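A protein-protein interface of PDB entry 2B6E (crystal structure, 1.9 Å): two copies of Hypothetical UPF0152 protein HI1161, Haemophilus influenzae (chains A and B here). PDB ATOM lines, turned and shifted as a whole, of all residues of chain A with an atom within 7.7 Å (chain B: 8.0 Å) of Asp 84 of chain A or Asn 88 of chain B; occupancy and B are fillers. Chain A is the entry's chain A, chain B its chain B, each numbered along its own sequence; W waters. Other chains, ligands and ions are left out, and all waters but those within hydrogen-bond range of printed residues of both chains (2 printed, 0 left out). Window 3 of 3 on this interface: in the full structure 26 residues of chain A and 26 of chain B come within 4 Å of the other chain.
ND1 of His 89 of chain B lies close to OE2 of Glu 63 of chain A, at 3.4 Å.
O of Leu 83 of chain A lies within hydrogen-bond range of N of His 89 of chain B (2.8 Å).
The backbone carbonyl oxygen (O) of Ile 85 of chain A is in hydrogen-bond range of the backbone NH (N) of Ala 87 of chain B.
N of Leu 83 of chain A sits at hydrogen-bond distance from O of Thr 132 of chain A.
The side-chain carboxylate (OD1) of Asp 84 of chain A sits at hydrogen-bond distance from the side-chain hydroxyl (OG1) of Thr 132 of chain A (2.9 Å).
The side-chain hydroxyl (OG) of Ser 129 of chain B sits at hydrogen-bond distance from the backbone carbonyl oxygen (O) of Asn 86 of chain B, 2.8 Å away.
N of Asn 86 of chain B sits at hydrogen-bond distance from O of Arg 130 of chain B (3.1 Å).
The side-chain sulfur of Cys 127 of chain B lies close to the backbone carbonyl oxygen of Asn 88 of chain B (3.7 Å).
The backbone carbonyl oxygen (O) of Val 128 of chain B sits at hydrogen-bond distance from the backbone NH (N) of Asn 88 of chain B (3.0 Å).
Among the printed residues, merely in contact across the chains: Asp 84 of chain A with Ala 87 of chain B, Ile 85 of chain A with Asn 86 of chain B, Leu 83 of chain A with Asn 88 of chain B, Asp 84 of chain A with Asn 88 of chain B, Glu 63 of chain A with Gly 55 of chain B, Asn 86 of chain A with Asn 86 of chain B and Gly 82 of chain A with His 89 of chain B.
Asn 88 of chain B touches two residues of chain A.
Of the printed residues of chain B, Ile 85 of chain A touches Asn 86 (3.2 Å) and Ala 87 (2.9 Å).
Printed residues of chain A within 4 Å of Gly 55 of chain B: Glu 63 (3.6 Å).
Printed residues of chain B within 4 Å of Asn 86 of chain A: Asn 86 (3.7 Å).
Ser 129 of chain B touches none of the printed residues of chain A.
The nearest residue of chain B that does not touch Asp 84 of chain A is His 89 of chain B (4.6 Å).
The nearest residue of chain A that does not touch Asn 88 of chain B is Ile 85 of chain A (5.2 Å).
Of the 16 printed residues of chain A, 6 touch a printed residue of chain B.
Along chain A the printed residues that touch a printed residue of chain B span positions 63 to 86.
Of the 17 printed residues of chain B, 5 touch a printed residue of chain A.
Hydrophobic or aromatic side chains of chain B within 4 Å of the printed part of chain A: His 89.
Among the printed residues, no Asp or Glu carboxylate lies within 4 Å of a Lys or Arg side-chain nitrogen of the other chain.
Asn 86 of chain B touches its own counterpart, Asn 86 of chain A.
Positions printed for both chains: 86, 129 and 130.
Of the 10 pairs that touch across the chains among the printed residues, 1 has its exchanged pair printed and touching as well.
Water W1 lies within hydrogen-bond range of the backbone carbonyl oxygen of Gly 82 of chain A (2.7 Å) and the backbone carbonyl oxygen of His 89 of chain B (2.8 Å).
Water W2 lies within hydrogen-bond range of the backbone carbonyl oxygen (O) of Leu 83 of chain A, the side-chain amide nitrogen (ND2) of Asn 88 of chain B and the backbone carbonyl oxygen (O) of His 89 of chain B.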
ATOM      1  N   GLU A  63      -3.752 -28.355   6.921  1.00  0.00           N
ATOM      2  CA  GLU A  63      -4.984 -27.780   7.438  1.00  0.00           C
ATOM      3  C   GLU A  63      -6.016 -27.589   6.329  1.00  0.00           C
ATOM      4  O   GLU A  63      -7.220 -27.758   6.553  1.00  0.00           O
ATOM      5  CB  GLU A  63      -4.726 -26.446   8.138  1.00  0.00           C
ATOM      6  CG  GLU A  63      -5.967 -25.957   8.861  1.00  0.00           C
ATOM      7  CD  GLU A  63      -5.665 -24.981   9.970  1.00  0.00           C
ATOM      8  OE1 GLU A  63      -4.557 -25.043  10.541  1.00  0.00           O
ATOM      9  OE2 GLU A  63      -6.553 -24.163  10.286  1.00  0.00           O
ATOM     10  N   VAL A  81     -14.588 -25.355  11.714  1.00  0.00           N
ATOM     11  CA  VAL A  81     -13.675 -24.277  12.062  1.00  0.00           C
ATOM     12  C   VAL A  81     -12.456 -24.969  12.667  1.00  0.00           C
ATOM     13  O   VAL A  81     -12.601 -25.821  13.543  1.00  0.00           O
ATOM     14  CB  VAL A  81     -14.287 -23.334  13.115  1.00  0.00           C
ATOM     15  CG1 VAL A  81     -13.288 -22.253  13.482  1.00  0.00           C
ATOM     16  CG2 VAL A  81     -15.562 -22.717  12.577  1.00  0.00           C
ATOM     17  N   GLY A  82     -11.266 -24.617  12.195  1.00  0.00           N
ATOM     18  CA  GLY A  82     -10.061 -25.232  12.721  1.00  0.00           C
ATOM     19  C   GLY A  82      -9.789 -24.759  14.137  1.00  0.00           C
ATOM     20  O   GLY A  82      -9.762 -23.556  14.395  1.00  0.00           O
ATOM     21  N   LEU A  83      -9.600 -25.695  15.060  1.00  0.00           N
ATOM     22  CA  LEU A  83      -9.329 -25.350  16.455  1.00  0.00           C
ATOM     23  C   LEU A  83      -7.823 -25.353  16.710  1.00  0.00           C
ATOM     24  O   LEU A  83      -7.255 -24.408  17.258  1.00  0.00           O
ATOM     25  CB  LEU A  83     -10.005 -26.371  17.379  1.00  0.00           C
ATOM     26  CG  LEU A  83     -11.249 -25.958  18.171  1.00  0.00           C
ATOM     27  CD1 LEU A  83     -12.101 -25.000  17.370  1.00  0.00           C
ATOM     28  CD2 LEU A  83     -12.025 -27.206  18.558  1.00  0.00           C
ATOM     29  N   ASP A  84      -7.175 -26.433  16.310  1.00  0.00           N
ATOM     30  CA  ASP A  84      -5.739 -26.540  16.506  1.00  0.00           C
ATOM     31  C   ASP A  84      -5.160 -27.572  15.566  1.00  0.00           C
ATOM     32  O   ASP A  84      -5.880 -28.392  15.006  1.00  0.00           O
ATOM     33  CB  ASP A  84      -5.418 -26.900  17.967  1.00  0.00           C
ATOM     34  CG  ASP A  84      -5.982 -28.252  18.386  1.00  0.00           C
ATOM     35  OD1 ASP A  84      -5.659 -29.260  17.728  1.00  0.00           O
ATOM     36  OD2 ASP A  84      -6.742 -28.305  19.385  1.00  0.00           O
ATOM     37  N   ILE A  85      -3.847 -27.533  15.394  1.00  0.00           N
ATOM     38  CA  ILE A  85      -3.201 -28.459  14.496  1.00  0.00           C
ATOM     39  C   ILE A  85      -1.750 -28.624  14.915  1.00  0.00           C
ATOM     40  O   ILE A  85      -1.147 -27.710  15.490  1.00  0.00           O
ATOM     41  CB  ILE A  85      -3.289 -27.927  13.038  1.00  0.00           C
ATOM     42  CG1 ILE A  85      -2.682 -28.933  12.059  1.00  0.00           C
ATOM     43  CG2 ILE A  85      -2.592 -26.578  12.931  1.00  0.00           C
ATOM     44  CD1 ILE A  85      -2.991 -28.603  10.613  1.00  0.00           C
ATOM     45  N   ASN A  86      -1.205 -29.807  14.664  1.00  0.00           N
ATOM     46  CA  ASN A  86       0.185 -30.069  14.990  1.00  0.00           C
ATOM     47  C   ASN A  86       0.779 -30.858  13.840  1.00  0.00           C
ATOM     48  O   ASN A  86       0.043 -31.379  12.994  1.00  0.00           O
ATOM     49  CB  ASN A  86       0.311 -30.829  16.323  1.00  0.00           C
ATOM     50  CG  ASN A  86      -0.403 -32.171  16.320  1.00  0.00           C
ATOM     51  OD1 ASN A  86      -0.106 -33.039  15.505  1.00  0.00           O
ATOM     52  ND2 ASN A  86      -1.341 -32.348  17.247  1.00  0.00           N
ATOM     53  N   GLN A 112     -14.328 -32.895  15.428  1.00  0.00           N
ATOM     54  CA  GLN A 112     -13.800 -33.860  14.477  1.00  0.00           C
ATOM     55  C   GLN A 112     -12.278 -33.860  14.608  1.00  0.00           C
ATOM     56  O   GLN A 112     -11.672 -32.819  14.854  1.00  0.00           O
ATOM     57  CB  GLN A 112     -14.157 -33.483  13.042  1.00  0.00           C
ATOM     58  CG  GLN A 112     -15.634 -33.524  12.697  1.00  0.00           C
ATOM     59  CD  GLN A 112     -15.872 -33.232  11.229  1.00  0.00           C
ATOM     60  OE1 GLN A 112     -17.004 -33.269  10.739  1.00  0.00           O
ATOM     61  NE2 GLN A 112     -14.794 -32.938  10.514  1.00  0.00           N
ATOM     62  N   VAL A 113     -11.667 -35.025  14.454  1.00  0.00           N
ATOM     63  CA  VAL A 113     -10.214 -35.131  14.518  1.00  0.00           C
ATOM     64  C   VAL A 113      -9.748 -35.812  13.240  1.00  0.00           C
ATOM     65  O   VAL A 113     -10.229 -36.895  12.883  1.00  0.00           O
ATOM     66  CB  VAL A 113      -9.748 -35.941  15.749  1.00  0.00           C
ATOM     67  CG1 VAL A 113      -8.218 -35.990  15.795  1.00  0.00           C
ATOM     68  CG2 VAL A 113     -10.285 -35.295  17.023  1.00  0.00           C
ATOM     69  N   TRP A 114      -8.824 -35.161  12.544  1.00  0.00           N
ATOM     70  CA  TRP A 114      -8.315 -35.676  11.287  1.00  0.00           C
ATOM     71  C   TRP A 114      -6.825 -35.949  11.263  1.00  0.00           C
ATOM     72  O   TRP A 114      -6.045 -35.243  11.906  1.00  0.00           O
ATOM     73  CB  TRP A 114      -8.650 -34.691  10.154  1.00  0.00           C
ATOM     74  CG  TRP A 114     -10.093 -34.673   9.774  1.00  0.00           C
ATOM     75  CD1 TRP A 114     -11.108 -34.003  10.397  1.00  0.00           C
ATOM     76  CD2 TRP A 114     -10.693 -35.410   8.707  1.00  0.00           C
ATOM     77  NE1 TRP A 114     -12.309 -34.283   9.780  1.00  0.00           N
ATOM     78  CE2 TRP A 114     -12.080 -35.148   8.741  1.00  0.00           C
ATOM     79  CE3 TRP A 114     -10.190 -36.277   7.723  1.00  0.00           C
ATOM     80  CZ2 TRP A 114     -12.972 -35.716   7.827  1.00  0.00           C
ATOM     81  CZ3 TRP A 114     -11.077 -36.843   6.813  1.00  0.00           C
ATOM     82  CH2 TRP A 114     -12.452 -36.562   6.875  1.00  0.00           C
ATOM     83  N   SER A 129       0.500 -34.948  10.331  1.00  0.00           N
ATOM     84  CA  SER A 129      -0.213 -33.908  11.053  1.00  0.00           C
ATOM     85  C   SER A 129      -1.547 -34.395  11.602  1.00  0.00           C
ATOM     86  O   SER A 129      -2.125 -35.358  11.092  1.00  0.00           O
ATOM     87  CB  SER A 129      -0.448 -32.733  10.090  1.00  0.00           C
ATOM     88  OG  SER A 129      -1.240 -31.711  10.667  1.00  0.00           O
ATOM     89  N   ARG A 130      -2.023 -33.742  12.661  1.00  0.00           N
ATOM     90  CA  ARG A 130      -3.325 -34.067  13.236  1.00  0.00           C
ATOM     91  C   ARG A 130      -4.036 -32.726  13.401  1.00  0.00           C
ATOM     92  O   ARG A 130      -3.441 -31.760  13.872  1.00  0.00           O
ATOM     93  CB  ARG A 130      -3.185 -34.786  14.583  1.00  0.00           C
ATOM     94  CG  ARG A 130      -4.441 -35.590  14.957  1.00  0.00           C
ATOM     95  CD  ARG A 130      -4.176 -36.554  16.114  1.00  0.00           C
ATOM     96  NE  ARG A 130      -3.764 -35.820  17.293  1.00  0.00           N
ATOM     97  CZ  ARG A 130      -2.615 -35.992  17.929  1.00  0.00           C
ATOM     98  NH1 ARG A 130      -1.732 -36.897  17.514  1.00  0.00           N
ATOM     99  NH2 ARG A 130      -2.336 -35.223  18.963  1.00  0.00           N
ATOM    100  N   LEU A 131      -5.301 -32.677  12.992  1.00  0.00           N
ATOM    101  CA  LEU A 131      -6.111 -31.466  13.029  1.00  0.00           C
ATOM    102  C   LEU A 131      -7.388 -31.659  13.840  1.00  0.00           C
ATOM    103  O   LEU A 131      -8.071 -32.665  13.690  1.00  0.00           O
ATOM    104  CB  LEU A 131      -6.486 -31.086  11.589  1.00  0.00           C
ATOM    105  CG  LEU A 131      -7.483 -29.966  11.262  1.00  0.00           C
ATOM    106  CD1 LEU A 131      -6.913 -28.607  11.609  1.00  0.00           C
ATOM    107  CD2 LEU A 131      -7.801 -30.036   9.764  1.00  0.00           C
ATOM    108  N   THR A 132      -7.707 -30.692  14.693  1.00  0.00           N
ATOM    109  CA  THR A 132      -8.918 -30.770  15.507  1.00  0.00           C
ATOM    110  C   THR A 132      -9.885 -29.694  15.010  1.00  0.00           C
ATOM    111  O   THR A 132      -9.534 -28.519  14.946  1.00  0.00           O
ATOM    112  CB  THR A 132      -8.602 -30.543  17.007  1.00  0.00           C
ATOM    113  OG1 THR A 132      -7.526 -31.408  17.401  1.00  0.00           O
ATOM    114  CG2 THR A 132      -9.825 -30.870  17.870  1.00  0.00           C
ATOM    115  N   LEU A 133     -11.099 -30.109  14.661  1.00  0.00           N
ATOM    116  CA  LEU A 133     -12.105 -29.191  14.141  1.00  0.00           C
ATOM    117  C   LEU A 133     -13.347 -29.141  15.005  1.00  0.00           C
ATOM    118  O   LEU A 133     -13.712 -30.120  15.652  1.00  0.00           O
ATOM    119  CB  LEU A 133     -12.541 -29.618  12.738  1.00  0.00           C
ATOM    120  CG  LEU A 133     -11.472 -29.853  11.673  1.00  0.00           C
ATOM    121  CD1 LEU A 133     -12.107 -30.529  10.462  1.00  0.00           C
ATOM    122  CD2 LEU A 133     -10.831 -28.525  11.285  1.00  0.00           C
ATOM    123  N   SER A 134     -13.998 -27.987  14.982  1.00  0.00           N
ATOM    124  CA  SER A 134     -15.235 -27.774  15.711  1.00  0.00           C
ATOM    125  C   SER A 134     -16.324 -27.736  14.647  1.00  0.00           C
ATOM    126  O   SER A 134     -16.132 -27.147  13.586  1.00  0.00           O
ATOM    127  CB  SER A 134     -15.185 -26.439  16.450  1.00  0.00           C
ATOM    128  OG  SER A 134     -16.388 -26.209  17.155  1.00  0.00           O
ATOM    129  N   GLY B  55      -5.885 -20.336   8.816  1.00  0.00           N
ATOM    130  CA  GLY B  55      -5.150 -20.841   9.962  1.00  0.00           C
ATOM    131  C   GLY B  55      -3.857 -21.561   9.628  1.00  0.00           C
ATOM    132  O   GLY B  55      -2.881 -21.455  10.367  1.00  0.00           O
ATOM    133  N   SER B  58      -1.217 -19.124   9.069  1.00  0.00           N
ATOM    134  CA  SER B  58      -0.764 -18.490  10.306  1.00  0.00           C
ATOM    135  C   SER B  58       0.370 -19.354  10.843  1.00  0.00           C
ATOM    136  O   SER B  58       1.375 -18.841  11.332  1.00  0.00           O
ATOM    137  CB  SER B  58      -1.884 -18.422  11.354  1.00  0.00           C
ATOM    138  OG  SER B  58      -2.960 -17.637  10.895  1.00  0.00           O
ATOM    139  N   VAL B  59       0.215 -20.672  10.742  1.00  0.00           N
ATOM    140  CA  VAL B  59       1.259 -21.570  11.217  1.00  0.00           C
ATOM    141  C   VAL B  59       2.520 -21.378  10.379  1.00  0.00           C
ATOM    142  O   VAL B  59       3.633 -21.437  10.902  1.00  0.00           O
ATOM    143  CB  VAL B  59       0.825 -23.048  11.146  1.00  0.00           C
ATOM    144  CG1 VAL B  59       1.954 -23.944  11.675  1.00  0.00           C
ATOM    145  CG2 VAL B  59      -0.437 -23.257  11.976  1.00  0.00           C
ATOM    146  N   ASN B  86       2.994 -26.860  16.606  1.00  0.00           N
ATOM    147  CA  ASN B  86       1.578 -26.989  16.905  1.00  0.00           C
ATOM    148  C   ASN B  86       1.036 -25.582  17.065  1.00  0.00           C
ATOM    149  O   ASN B  86       1.802 -24.633  17.218  1.00  0.00           O
ATOM    150  CB  ASN B  86       1.343 -27.823  18.177  1.00  0.00           C
ATOM    151  CG  ASN B  86       2.025 -27.244  19.403  1.00  0.00           C
ATOM    152  OD1 ASN B  86       1.739 -26.121  19.819  1.00  0.00           O
ATOM    153  ND2 ASN B  86       2.937 -28.013  19.987  1.00  0.00           N
ATOM    154  N   ALA B  87      -0.279 -25.440  17.005  1.00  0.00           N
ATOM    155  CA  ALA B  87      -0.888 -24.132  17.135  1.00  0.00           C
ATOM    156  C   ALA B  87      -2.375 -24.251  17.415  1.00  0.00           C
ATOM    157  O   ALA B  87      -3.016 -25.232  17.025  1.00  0.00           O
ATOM    158  CB  ALA B  87      -0.671 -23.335  15.846  1.00  0.00           C
ATOM    159  N   ASN B  88      -2.904 -23.255  18.119  1.00  0.00           N
ATOM    160  CA  ASN B  88      -4.328 -23.172  18.414  1.00  0.00           C
ATOM    161  C   ASN B  88      -4.787 -21.872  17.781  1.00  0.00           C
ATOM    162  O   ASN B  88      -4.167 -20.821  17.984  1.00  0.00           O
ATOM    163  CB  ASN B  88      -4.607 -23.108  19.919  1.00  0.00           C
ATOM    164  CG  ASN B  88      -4.693 -24.475  20.555  1.00  0.00           C
ATOM    165  OD1 ASN B  88      -3.687 -25.164  20.700  1.00  0.00           O
ATOM    166  ND2 ASN B  88      -5.906 -24.882  20.928  1.00  0.00           N
ATOM    167  N   HIS B  89      -5.860 -21.942  17.000  1.00  0.00           N
ATOM    168  CA  HIS B  89      -6.411 -20.759  16.350  1.00  0.00           C
ATOM    169  C   HIS B  89      -7.483 -20.262  17.304  1.00  0.00           C
ATOM    170  O   HIS B  89      -8.448 -20.973  17.594  1.00  0.00           O
ATOM    171  CB  HIS B  89      -6.981 -21.156  14.987  1.00  0.00           C
ATOM    172  CG  HIS B  89      -5.953 -21.763  14.084  1.00  0.00           C
ATOM    173  ND1 HIS B  89      -6.125 -22.984  13.465  1.00  0.00           N
ATOM    174  CD2 HIS B  89      -4.715 -21.339  13.740  1.00  0.00           C
ATOM    175  CE1 HIS B  89      -5.036 -23.284  12.781  1.00  0.00           C
ATOM    176  NE2 HIS B  89      -4.164 -22.303  12.930  1.00  0.00           N
ATOM    177  N   LEU B  90      -7.294 -19.043  17.799  1.00  0.00           N
ATOM    178  CA  LEU B  90      -8.191 -18.477  18.795  1.00  0.00           C
ATOM    179  C   LEU B  90      -9.359 -17.658  18.291  1.00  0.00           C
ATOM    180  O   LEU B  90     -10.420 -17.652  18.909  1.00  0.00           O
ATOM    181  CB  LEU B  90      -7.374 -17.641  19.781  1.00  0.00           C
ATOM    182  CG  LEU B  90      -6.119 -18.342  20.301  1.00  0.00           C
ATOM    183  CD1 LEU B  90      -5.357 -17.411  21.233  1.00  0.00           C
ATOM    184  CD2 LEU B  90      -6.510 -19.639  21.017  1.00  0.00           C
ATOM    185  N   ARG B  91      -9.174 -16.961  17.179  1.00  0.00           N
ATOM    186  CA  ARG B  91     -10.249 -16.140  16.646  1.00  0.00           C
ATOM    187  C   ARG B  91     -10.006 -15.803  15.189  1.00  0.00           C
ATOM    188  O   ARG B  91      -8.865 -15.799  14.725  1.00  0.00           O
ATOM    189  CB  ARG B  91     -10.363 -14.847  17.448  1.00  0.00           C
ATOM    190  CG  ARG B  91      -9.149 -13.943  17.349  1.00  0.00           C
ATOM    191  CD  ARG B  91      -9.398 -12.645  18.096  1.00  0.00           C
ATOM    192  NE  ARG B  91      -9.595 -12.879  19.525  1.00  0.00           N
ATOM    193  CZ  ARG B  91     -10.219 -12.038  20.344  1.00  0.00           C
ATOM    194  NH1 ARG B  91     -10.717 -10.897  19.880  1.00  0.00           N
ATOM    195  NH2 ARG B  91     -10.344 -12.336  21.631  1.00  0.00           N
ATOM    196  N   ILE B 116       5.560 -18.792  19.779  1.00  0.00           N
ATOM    197  CA  ILE B 116       5.215 -17.784  18.784  1.00  0.00           C
ATOM    198  C   ILE B 116       3.754 -17.397  18.955  1.00  0.00           C
ATOM    199  O   ILE B 116       2.853 -18.222  18.780  1.00  0.00           O
ATOM    200  CB  ILE B 116       5.411 -18.259  17.328  1.00  0.00           C
ATOM    201  CG1 ILE B 116       6.850 -18.726  17.097  1.00  0.00           C
ATOM    202  CG2 ILE B 116       5.106 -17.092  16.370  1.00  0.00           C
ATOM    203  CD1 ILE B 116       7.061 -20.208  17.358  1.00  0.00           C
ATOM    204  N   ILE B 118       0.702 -14.778  17.778  1.00  0.00           N
ATOM    205  CA  ILE B 118       0.298 -13.916  16.670  1.00  0.00           C
ATOM    206  C   ILE B 118      -0.864 -13.029  17.097  1.00  0.00           C
ATOM    207  O   ILE B 118      -1.871 -13.517  17.619  1.00  0.00           O
ATOM    208  CB  ILE B 118      -0.100 -14.779  15.451  1.00  0.00           C
ATOM    209  CG1 ILE B 118       1.040 -15.756  15.140  1.00  0.00           C
ATOM    210  CG2 ILE B 118      -0.345 -13.901  14.222  1.00  0.00           C
ATOM    211  CD1 ILE B 118       0.767 -16.666  13.954  1.00  0.00           C
ATOM    212  N   LEU B 125      -4.922 -11.427  20.482  1.00  0.00           N
ATOM    213  CA  LEU B 125      -4.259 -12.690  20.181  1.00  0.00           C
ATOM    214  C   LEU B 125      -5.135 -13.570  19.284  1.00  0.00           C
ATOM    215  O   LEU B 125      -6.262 -13.907  19.652  1.00  0.00           O
ATOM    216  CB  LEU B 125      -3.957 -13.405  21.498  1.00  0.00           C
ATOM    217  CG  LEU B 125      -2.912 -14.511  21.564  1.00  0.00           C
ATOM    218  CD1 LEU B 125      -1.543 -13.954  21.207  1.00  0.00           C
ATOM    219  CD2 LEU B 125      -2.899 -15.087  22.983  1.00  0.00           C
ATOM    220  N   CYS B 126      -4.637 -13.939  18.106  1.00  0.00           N
ATOM    221  CA  CYS B 126      -5.430 -14.784  17.210  1.00  0.00           C
ATOM    222  C   CYS B 126      -4.866 -16.195  17.048  1.00  0.00           C
ATOM    223  O   CYS B 126      -5.561 -17.095  16.577  1.00  0.00           O
ATOM    224  CB  CYS B 126      -5.576 -14.130  15.828  1.00  0.00           C
ATOM    225  SG  CYS B 126      -4.031 -13.883  14.902  1.00  0.00           S
ATOM    226  N   CYS B 127      -3.613 -16.390  17.442  1.00  0.00           N
ATOM    227  CA  CYS B 127      -2.981 -17.702  17.319  1.00  0.00           C
ATOM    228  C   CYS B 127      -1.804 -17.842  18.281  1.00  0.00           C
ATOM    229  O   CYS B 127      -1.047 -16.890  18.493  1.00  0.00           O
ATOM    230  CB  CYS B 127      -2.497 -17.909  15.874  1.00  0.00           C
ATOM    231  SG  CYS B 127      -1.766 -19.539  15.476  1.00  0.00           S
ATOM    232  N   VAL B 128      -1.674 -19.021  18.886  1.00  0.00           N
ATOM    233  CA  VAL B 128      -0.560 -19.310  19.782  1.00  0.00           C
ATOM    234  C   VAL B 128       0.074 -20.578  19.220  1.00  0.00           C
ATOM    235  O   VAL B 128      -0.625 -21.523  18.863  1.00  0.00           O
ATOM    236  CB  VAL B 128      -1.010 -19.534  21.254  1.00  0.00           C
ATOM    237  CG1 VAL B 128      -1.462 -18.203  21.854  1.00  0.00           C
ATOM    238  CG2 VAL B 128      -2.135 -20.560  21.333  1.00  0.00           C
ATOM    239  N   SER B 129       1.396 -20.589  19.138  1.00  0.00           N
ATOM    240  CA  SER B 129       2.111 -21.716  18.562  1.00  0.00           C
ATOM    241  C   SER B 129       3.398 -22.050  19.305  1.00  0.00           C
ATOM    242  O   SER B 129       3.993 -21.191  19.959  1.00  0.00           O
ATOM    243  CB  SER B 129       2.435 -21.381  17.096  1.00  0.00           C
ATOM    244  OG  SER B 129       3.280 -22.354  16.489  1.00  0.00           O
ATOM    245  N   ARG B 130       3.820 -23.307  19.226  1.00  0.00           N
ATOM    246  CA  ARG B 130       5.080 -23.705  19.844  1.00  0.00           C
ATOM    247  C   ARG B 130       5.834 -24.489  18.786  1.00  0.00           C
ATOM    248  O   ARG B 130       5.265 -25.360  18.123  1.00  0.00           O
ATOM    249  CB  ARG B 130       4.873 -24.563  21.100  1.00  0.00           C
ATOM    250  CG  ARG B 130       6.143 -24.661  21.958  1.00  0.00           C
ATOM    251  CD  ARG B 130       5.847 -25.234  23.346  1.00  0.00           C
ATOM    252  NE  ARG B 130       5.356 -26.594  23.228  1.00  0.00           N
ATOM    253  CZ  ARG B 130       4.131 -26.989  23.556  1.00  0.00           C
ATOM    254  NH1 ARG B 130       3.240 -26.130  24.046  1.00  0.00           N
ATOM    255  NH2 ARG B 130       3.794 -28.245  23.355  1.00  0.00           N
HETATM  256  O   HOH W   1     -10.677 -21.614  16.010  1.00  0.00           O
HETATM  257  O   HOH W   2      -8.228 -23.475  19.786  1.00  0.00           O
